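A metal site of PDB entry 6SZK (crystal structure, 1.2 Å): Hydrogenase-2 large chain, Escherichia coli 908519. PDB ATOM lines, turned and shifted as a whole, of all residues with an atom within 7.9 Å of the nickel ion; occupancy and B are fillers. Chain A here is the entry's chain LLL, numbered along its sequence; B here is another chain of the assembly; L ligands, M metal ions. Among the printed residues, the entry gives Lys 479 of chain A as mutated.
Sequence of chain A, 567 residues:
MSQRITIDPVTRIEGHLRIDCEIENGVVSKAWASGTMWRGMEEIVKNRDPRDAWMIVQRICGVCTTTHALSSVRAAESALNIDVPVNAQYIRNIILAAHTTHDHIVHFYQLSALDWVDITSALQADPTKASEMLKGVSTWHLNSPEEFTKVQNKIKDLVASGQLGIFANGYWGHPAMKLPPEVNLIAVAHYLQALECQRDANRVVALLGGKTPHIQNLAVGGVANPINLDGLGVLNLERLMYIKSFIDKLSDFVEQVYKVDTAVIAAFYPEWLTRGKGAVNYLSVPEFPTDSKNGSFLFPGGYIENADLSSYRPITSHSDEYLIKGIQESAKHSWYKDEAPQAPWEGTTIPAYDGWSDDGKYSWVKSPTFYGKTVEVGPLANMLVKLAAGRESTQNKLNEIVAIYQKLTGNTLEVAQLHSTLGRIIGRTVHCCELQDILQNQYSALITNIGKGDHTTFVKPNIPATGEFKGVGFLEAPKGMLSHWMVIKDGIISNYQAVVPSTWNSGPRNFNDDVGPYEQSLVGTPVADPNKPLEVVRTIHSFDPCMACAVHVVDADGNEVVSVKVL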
ATOM      1  N   GLU A  14     -24.451 -12.308 -30.215  1.00  0.00           N
ATOM      2  CA  GLU A  14     -25.286 -12.762 -29.092  1.00  0.00           C
ATOM      3  C   GLU A  14     -26.739 -12.494 -29.368  1.00  0.00           C
ATOM      4  O   GLU A  14     -27.165 -11.353 -29.676  1.00  0.00           O
ATOM      5  CB  GLU A  14     -24.837 -12.130 -27.749  1.00  0.00           C
ATOM      6  CG  GLU A  14     -25.481 -12.754 -26.504  1.00  0.00           C
ATOM      7  CD  GLU A  14     -26.977 -12.669 -26.406  1.00  0.00           C
ATOM      8  OE1 GLU A  14     -27.574 -11.655 -26.775  1.00  0.00           O
ATOM      9  OE2 GLU A  14     -27.640 -13.669 -25.869  1.00  0.00           O
ATOM     10  N   ILE A  60     -29.001 -10.745 -17.454  1.00  0.00           N
ATOM     11  CA  ILE A  60     -29.331 -10.081 -18.728  1.00  0.00           C
ATOM     12  C   ILE A  60     -28.417 -10.663 -19.841  1.00  0.00           C
ATOM     13  O   ILE A  60     -28.915 -10.877 -21.007  1.00  0.00           O
ATOM     14  CB  ILE A  60     -29.207  -8.532 -18.648  1.00  0.00           C
ATOM     15  CG1 ILE A  60     -30.392  -7.979 -17.814  1.00  0.00           C
ATOM     16  CG2 ILE A  60     -29.123  -7.891 -20.025  1.00  0.00           C
ATOM     17  CD1 ILE A  60     -30.313  -6.493 -17.466  1.00  0.00           C
ATOM     18  N   CYS A  61     -27.134 -10.945 -19.566  1.00  0.00           N
ATOM     19  CA  CYS A  61     -26.220 -11.430 -20.637  1.00  0.00           C
ATOM     20  C   CYS A  61     -25.066 -12.231 -20.048  1.00  0.00           C
ATOM     21  O   CYS A  61     -24.410 -11.773 -19.087  1.00  0.00           O
ATOM     22  CB  CYS A  61     -25.689 -10.235 -21.450  1.00  0.00           C
ATOM     23  SG  CYS A  61     -24.755 -10.728 -22.920  1.00  0.00           S
ATOM     24  N   GLY A  62     -24.763 -13.367 -20.718  1.00  0.00           N
ATOM     25  CA  GLY A  62     -23.616 -14.179 -20.375  1.00  0.00           C
ATOM     26  C   GLY A  62     -22.401 -14.003 -21.257  1.00  0.00           C
ATOM     27  O   GLY A  62     -21.329 -14.594 -20.942  1.00  0.00           O
ATOM     28  N   VAL A  63     -22.525 -13.274 -22.394  1.00  0.00           N
ATOM     29  CA  VAL A  63     -21.356 -12.865 -23.182  1.00  0.00           C
ATOM     30  C   VAL A  63     -20.672 -11.720 -22.427  1.00  0.00           C
ATOM     31  O   VAL A  63     -19.490 -11.862 -21.963  1.00  0.00           O
ATOM     32  CB  VAL A  63     -21.664 -12.504 -24.656  1.00  0.00           C
ATOM     33  CG1 VAL A  63     -20.357 -12.044 -25.346  1.00  0.00           C
ATOM     34  CG2 VAL A  63     -22.270 -13.734 -25.345  1.00  0.00           C
ATOM     35  N   CYS A  64     -21.393 -10.633 -22.196  1.00  0.00           N
ATOM     36  CA  CYS A  64     -20.909  -9.513 -21.342  1.00  0.00           C
ATOM     37  C   CYS A  64     -21.313  -9.788 -19.896  1.00  0.00           C
ATOM     38  O   CYS A  64     -21.827  -8.947 -19.146  1.00  0.00           O
ATOM     39  CB  CYS A  64     -21.375  -8.149 -21.889  1.00  0.00           C
ATOM     40  SG  CYS A  64     -23.136  -7.849 -21.847  1.00  0.00           S
ATOM     41  N   THR A  65     -20.957 -11.016 -19.417  1.00  0.00           N
ATOM     42  CA  THR A  65     -21.022 -11.355 -17.973  1.00  0.00           C
ATOM     43  C   THR A  65     -20.121 -10.338 -17.207  1.00  0.00           C
ATOM     44  O   THR A  65     -19.266  -9.654 -17.837  1.00  0.00           O
ATOM     45  CB  THR A  65     -20.718 -12.835 -17.740  1.00  0.00           C
ATOM     46  OG1 THR A  65     -21.016 -13.155 -16.363  1.00  0.00           O
ATOM     47  CG2 THR A  65     -19.264 -13.195 -17.993  1.00  0.00           C
ATOM     48  N   THR A  67     -20.745  -7.359 -16.330  1.00  0.00           N
ATOM     49  CA  THR A  67     -21.005  -5.925 -16.577  1.00  0.00           C
ATOM     50  C   THR A  67     -22.310  -5.447 -15.856  1.00  0.00           C
ATOM     51  O   THR A  67     -22.318  -4.389 -15.223  1.00  0.00           O
ATOM     52  CB  THR A  67     -21.084  -5.601 -18.091  1.00  0.00           C
ATOM     53  OG1 THR A  67     -22.190  -6.173 -18.753  1.00  0.00           O
ATOM     54  CG2 THR A  67     -19.763  -5.933 -18.787  1.00  0.00           C
ATOM     55  N   HIS A  68     -23.377  -6.226 -16.013  1.00  0.00           N
ATOM     56  CA  HIS A  68     -24.662  -5.827 -15.391  1.00  0.00           C
ATOM     57  C   HIS A  68     -24.629  -6.017 -13.874  1.00  0.00           C
ATOM     58  O   HIS A  68     -25.318  -5.278 -13.132  1.00  0.00           O
ATOM     59  CB  HIS A  68     -25.813  -6.662 -16.032  1.00  0.00           C
ATOM     60  CG  HIS A  68     -26.051  -6.315 -17.458  1.00  0.00           C
ATOM     61  ND1 HIS A  68     -26.695  -5.138 -17.857  1.00  0.00           N
ATOM     62  CD2 HIS A  68     -25.687  -6.991 -18.578  1.00  0.00           C
ATOM     63  CE1 HIS A  68     -26.682  -5.127 -19.185  1.00  0.00           C
ATOM     64  NE2 HIS A  68     -26.077  -6.243 -19.680  1.00  0.00           N
ATOM     65  N   HIS A  99     -12.118  -9.525 -18.118  1.00  0.00           N
ATOM     66  CA  HIS A  99     -13.322  -9.959 -18.864  1.00  0.00           C
ATOM     67  C   HIS A  99     -13.360  -9.310 -20.278  1.00  0.00           C
ATOM     68  O   HIS A  99     -13.581 -10.013 -21.316  1.00  0.00           O
ATOM     69  CB  HIS A  99     -14.646  -9.603 -18.116  1.00  0.00           C
ATOM     70  CG  HIS A  99     -15.798  -9.888 -19.047  1.00  0.00           C
ATOM     71  ND1 HIS A  99     -16.263 -11.158 -19.276  1.00  0.00           N
ATOM     72  CD2 HIS A  99     -16.368  -9.054 -19.978  1.00  0.00           C
ATOM     73  CE1 HIS A  99     -17.139 -11.101 -20.295  1.00  0.00           C
ATOM     74  NE2 HIS A  99     -17.158  -9.827 -20.807  1.00  0.00           N
ATOM     75  N   ASP A 103     -13.560 -10.802 -24.121  1.00  0.00           N
ATOM     76  CA  ASP A 103     -14.731 -10.456 -24.953  1.00  0.00           C
ATOM     77  C   ASP A 103     -14.262  -9.917 -26.341  1.00  0.00           C
ATOM     78  O   ASP A 103     -14.746 -10.395 -27.406  1.00  0.00           O
ATOM     79  CB  ASP A 103     -15.506  -9.387 -24.164  1.00  0.00           C
ATOM     80  CG  ASP A 103     -16.933  -9.186 -24.471  1.00  0.00           C
ATOM     81  OD1 ASP A 103     -17.151  -8.929 -25.699  1.00  0.00           O
ATOM     82  OD2 ASP A 103     -17.804  -9.082 -23.525  1.00  0.00           O
ATOM     83  N   ALA A 477     -18.801  -0.607 -20.737  1.00  0.00           N
ATOM     84  CA  ALA A 477     -18.809  -2.034 -21.047  1.00  0.00           C
ATOM     85  C   ALA A 477     -18.073  -2.277 -22.355  1.00  0.00           C
ATOM     86  O   ALA A 477     -17.772  -1.391 -23.140  1.00  0.00           O
ATOM     87  CB  ALA A 477     -20.239  -2.553 -21.072  1.00  0.00           C
ATOM     88  N   PRO A 478     -17.825  -3.586 -22.683  1.00  0.00           N
ATOM     89  CA  PRO A 478     -17.160  -3.900 -23.955  1.00  0.00           C
ATOM     90  C   PRO A 478     -17.877  -3.349 -25.233  1.00  0.00           C
ATOM     91  O   PRO A 478     -17.212  -3.012 -26.213  1.00  0.00           O
ATOM     92  CB  PRO A 478     -17.079  -5.476 -23.977  1.00  0.00           C
ATOM     93  CG  PRO A 478     -16.997  -5.808 -22.499  1.00  0.00           C
ATOM     94  CD  PRO A 478     -17.944  -4.815 -21.826  1.00  0.00           C
ATOM     95  N   LYS A 479     -19.230  -3.276 -25.182  1.00  0.00           N
ATOM     96  CA  LYS A 479     -20.033  -2.736 -26.287  1.00  0.00           C
ATOM     97  C   LYS A 479     -20.359  -1.247 -26.096  1.00  0.00           C
ATOM     98  O   LYS A 479     -20.973  -0.670 -27.044  1.00  0.00           O
ATOM     99  CB  LYS A 479     -21.337  -3.527 -26.493  1.00  0.00           C
ATOM    100  CG  LYS A 479     -21.312  -4.687 -27.471  1.00  0.00           C
ATOM    101  CD  LYS A 479     -21.182  -6.119 -26.918  1.00  0.00           C
ATOM    102  CE  LYS A 479     -19.867  -6.504 -26.300  1.00  0.00           C
ATOM    103  NZ  LYS A 479     -19.542  -7.965 -26.549  1.00  0.00           N
ATOM    104  N   VAL A 500     -28.871  -0.046 -22.219  1.00  0.00           N
ATOM    105  CA  VAL A 500     -27.714  -0.912 -22.466  1.00  0.00           C
ATOM    106  C   VAL A 500     -27.014  -0.494 -23.770  1.00  0.00           C
ATOM    107  O   VAL A 500     -27.696   0.081 -24.654  1.00  0.00           O
ATOM    108  CB  VAL A 500     -28.183  -2.381 -22.446  1.00  0.00           C
ATOM    109  CG1 VAL A 500     -27.042  -3.405 -22.470  1.00  0.00           C
ATOM    110  CG2 VAL A 500     -29.012  -2.666 -21.138  1.00  0.00           C
ATOM    111  N   PRO A 501     -25.679  -0.658 -23.962  1.00  0.00           N
ATOM    112  CA  PRO A 501     -25.049  -0.074 -25.161  1.00  0.00           C
ATOM    113  C   PRO A 501     -25.650  -0.557 -26.464  1.00  0.00           C
ATOM    114  O   PRO A 501     -25.923   0.268 -27.380  1.00  0.00           O
ATOM    115  CB  PRO A 501     -23.544  -0.420 -25.036  1.00  0.00           C
ATOM    116  CG  PRO A 501     -23.461  -1.419 -23.915  1.00  0.00           C
ATOM    117  CD  PRO A 501     -24.651  -1.108 -22.990  1.00  0.00           C
ATOM    118  N   SER A 502     -25.995  -1.856 -26.610  1.00  0.00           N
ATOM    119  CA  SER A 502     -26.640  -2.321 -27.866  1.00  0.00           C
ATOM    120  C   SER A 502     -28.054  -1.728 -28.018  1.00  0.00           C
ATOM    121  O   SER A 502     -28.587  -1.700 -29.141  1.00  0.00           O
ATOM    122  CB  SER A 502     -26.640  -3.852 -28.014  1.00  0.00           C
ATOM    123  OG  SER A 502     -25.326  -4.376 -28.223  1.00  0.00           O
ATOM    124  N   ASP A 544     -20.663  -5.315 -32.891  1.00  0.00           N
ATOM    125  CA  ASP A 544     -20.694  -6.387 -31.867  1.00  0.00           C
ATOM    126  C   ASP A 544     -22.087  -6.468 -31.210  1.00  0.00           C
ATOM    127  O   ASP A 544     -22.290  -6.331 -29.982  1.00  0.00           O
ATOM    128  CB  ASP A 544     -19.564  -6.098 -30.851  1.00  0.00           C
ATOM    129  CG  ASP A 544     -19.228  -7.130 -29.826  1.00  0.00           C
ATOM    130  OD1 ASP A 544     -19.759  -8.296 -29.896  1.00  0.00           O
ATOM    131  OD2 ASP A 544     -18.376  -6.802 -28.956  1.00  0.00           O
ATOM    132  N   PRO A 545     -23.132  -6.799 -32.034  1.00  0.00           N
ATOM    133  CA  PRO A 545     -24.502  -6.884 -31.486  1.00  0.00           C
ATOM    134  C   PRO A 545     -24.656  -7.861 -30.309  1.00  0.00           C
ATOM    135  O   PRO A 545     -24.199  -9.012 -30.355  1.00  0.00           O
ATOM    136  CB  PRO A 545     -25.378  -7.303 -32.665  1.00  0.00           C
ATOM    137  CG  PRO A 545     -24.570  -6.874 -33.887  1.00  0.00           C
ATOM    138  CD  PRO A 545     -23.136  -7.129 -33.497  1.00  0.00           C
ATOM    139  N   CYS A 546     -25.402  -7.410 -29.284  1.00  0.00           N
ATOM    140  CA  CYS A 546     -25.796  -8.244 -28.131  1.00  0.00           C
ATOM    141  C   CYS A 546     -27.333  -7.990 -27.884  1.00  0.00           C
ATOM    142  O   CYS A 546     -27.695  -6.928 -27.358  1.00  0.00           O
ATOM    143  CB  CYS A 546     -24.955  -7.973 -26.905  1.00  0.00           C
ATOM    144  SG  CYS A 546     -25.405  -9.127 -25.575  1.00  0.00           S
ATOM    145  N   MET A 547     -28.185  -8.945 -28.327  1.00  0.00           N
ATOM    146  CA  MET A 547     -29.646  -8.639 -28.302  1.00  0.00           C
ATOM    147  C   MET A 547     -30.269  -9.017 -26.948  1.00  0.00           C
ATOM    148  O   MET A 547     -31.344  -8.419 -26.601  1.00  0.00           O
ATOM    149  CB  MET A 547     -30.364  -9.337 -29.477  1.00  0.00           C
ATOM    150  CG  MET A 547     -29.763  -8.943 -30.845  1.00  0.00           C
ATOM    151  SD  MET A 547     -29.462  -7.163 -31.108  1.00  0.00           S
ATOM    152  CE  MET A 547     -31.109  -6.572 -31.080  1.00  0.00           C
ATOM    153  N   ALA A 548     -29.715  -9.965 -26.186  1.00  0.00           N
ATOM    154  CA  ALA A 548     -30.114 -10.166 -24.774  1.00  0.00           C
ATOM    155  C   ALA A 548     -29.860  -8.850 -23.990  1.00  0.00           C
ATOM    156  O   ALA A 548     -30.759  -8.364 -23.234  1.00  0.00           O
ATOM    157  CB  ALA A 548     -29.363 -11.364 -24.151  1.00  0.00           C
ATOM    158  N   CYS A 549     -28.686  -8.252 -24.213  1.00  0.00           N
ATOM    159  CA  CYS A 549     -28.406  -6.893 -23.691  1.00  0.00           C
ATOM    160  C   CYS A 549     -29.407  -5.839 -24.222  1.00  0.00           C
ATOM    161  O   CYS A 549     -29.918  -5.033 -23.450  1.00  0.00           O
ATOM    162  CB  CYS A 549     -26.963  -6.523 -24.058  1.00  0.00           C
ATOM    163  SG  CYS A 549     -25.753  -7.082 -22.861  1.00  0.00           S
ATOM    164  N   ALA A 550     -29.588  -5.782 -25.558  1.00  0.00           N
ATOM    165  CA  ALA A 550     -30.362  -4.656 -26.136  1.00  0.00           C
ATOM    166  C   ALA A 550     -31.782  -4.629 -25.580  1.00  0.00           C
ATOM    167  O   ALA A 550     -32.356  -3.551 -25.357  1.00  0.00           O
ATOM    168  CB  ALA A 550     -30.396  -4.753 -27.643  1.00  0.00           C
ATOM    169  N   CYS B  21     -29.353 -16.327 -22.226  1.00  0.00           N
ATOM    170  CA  CYS B  21     -28.428 -15.200 -22.087  1.00  0.00           C
ATOM    171  C   CYS B  21     -27.041 -15.447 -22.794  1.00  0.00           C
ATOM    172  O   CYS B  21     -26.210 -14.536 -22.837  1.00  0.00           O
ATOM    173  CB  CYS B  21     -28.136 -14.829 -20.605  1.00  0.00           C
ATOM    174  SG  CYS B  21     -26.971 -15.921 -19.761  1.00  0.00           S
ATOM    175  N   THR B  22     -26.850 -16.711 -23.269  1.00  0.00           N
ATOM    176  CA  THR B  22     -25.597 -17.225 -23.946  1.00  0.00           C
ATOM    177  C   THR B  22     -24.543 -17.703 -22.960  1.00  0.00           C
ATOM    178  O   THR B  22     -23.527 -18.277 -23.383  1.00  0.00           O
ATOM    179  CB  THR B  22     -25.120 -16.269 -25.053  1.00  0.00           C
ATOM    180  OG1 THR B  22     -26.252 -15.873 -25.848  1.00  0.00           O
ATOM    181  CG2 THR B  22     -24.066 -16.857 -26.002  1.00  0.00           C
HETATM  182  C1  LIG L   1     -22.618  -8.838 -24.849  1.00  0.00           C
HETATM  183  O1  LIG L   1     -21.765  -9.152 -25.558  1.00  0.00           O
HETATM  184 FE1  LG2 L   2     -23.713  -6.048 -23.099  1.00  0.00          FE
HETATM  185  C1  LG2 L   2     -24.289  -5.099 -24.539  1.00  0.00           C
HETATM  186  N1  LG2 L   2     -24.689  -4.414 -25.473  1.00  0.00           N
HETATM  187  C2  LG2 L   2     -21.944  -5.506 -23.360  1.00  0.00           C
HETATM  188  N2  LG2 L   2     -20.824  -5.131 -23.438  1.00  0.00           N
HETATM  189  C3  LG2 L   2     -23.813  -4.755 -21.914  1.00  0.00           C
HETATM  190  O1  LG2 L   2     -23.838  -3.882 -21.151  1.00  0.00           O
HETATM  191 NI    NI M   1     -24.195  -8.559 -23.750  1.00  0.00          NI
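The side-chain carboxylate of Glu 14 sits close to the side-chain sulfur of Cys 546.
The backbone NH (N) of Cys 546 is in hydrogen-bond range of the side-chain hydroxyl (OG) of Ser 502.
O of Cys 64 lies within hydrogen-bond range of OG1 of Thr 67, at 2.8 Å.
NE2 of His 68 sits close to SG of Cys 549, at 3.3 Å.
N of Val 63 sits close to SG of Cys 61.
An oxygen (O1) of LIG L1 sits close to the side-chain sulfur (SG) of Cys 546.
O1 of LIG L1 lies within hydrogen-bond range of NZ of Lys 479 (2.7 Å).
FE1 of LG2 L2 is bound by SG of Cys 64.
FE1 of LG2 L2 is bound by SG of Cys 549 (2.3 Å).
The backbone NH (N) of Lys 479 lies within hydrogen-bond range of a nitrogen (N2) of LG2 L2 (3.0 Å).
The backbone NH of Ser 502 is in hydrogen-bond range of a nitrogen (N1) of LG2 L2 (3.1 Å).
OG of Ser 502 sits at hydrogen-bond distance from N1 of LG2 L2, at 2.8 Å.
Of the 26 residues printed, 4 come within 4 Å of the nickel ion.
Along chain A the residues within 4 Å of the nickel ion span positions 61 to 549.
The nickel ion is bound by SG of Cys 546 (2.3 Å), SG of Cys 64 (2.3 Å), SG of Cys 549 (2.3 Å) and SG of Cys 61 (2.4 Å).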
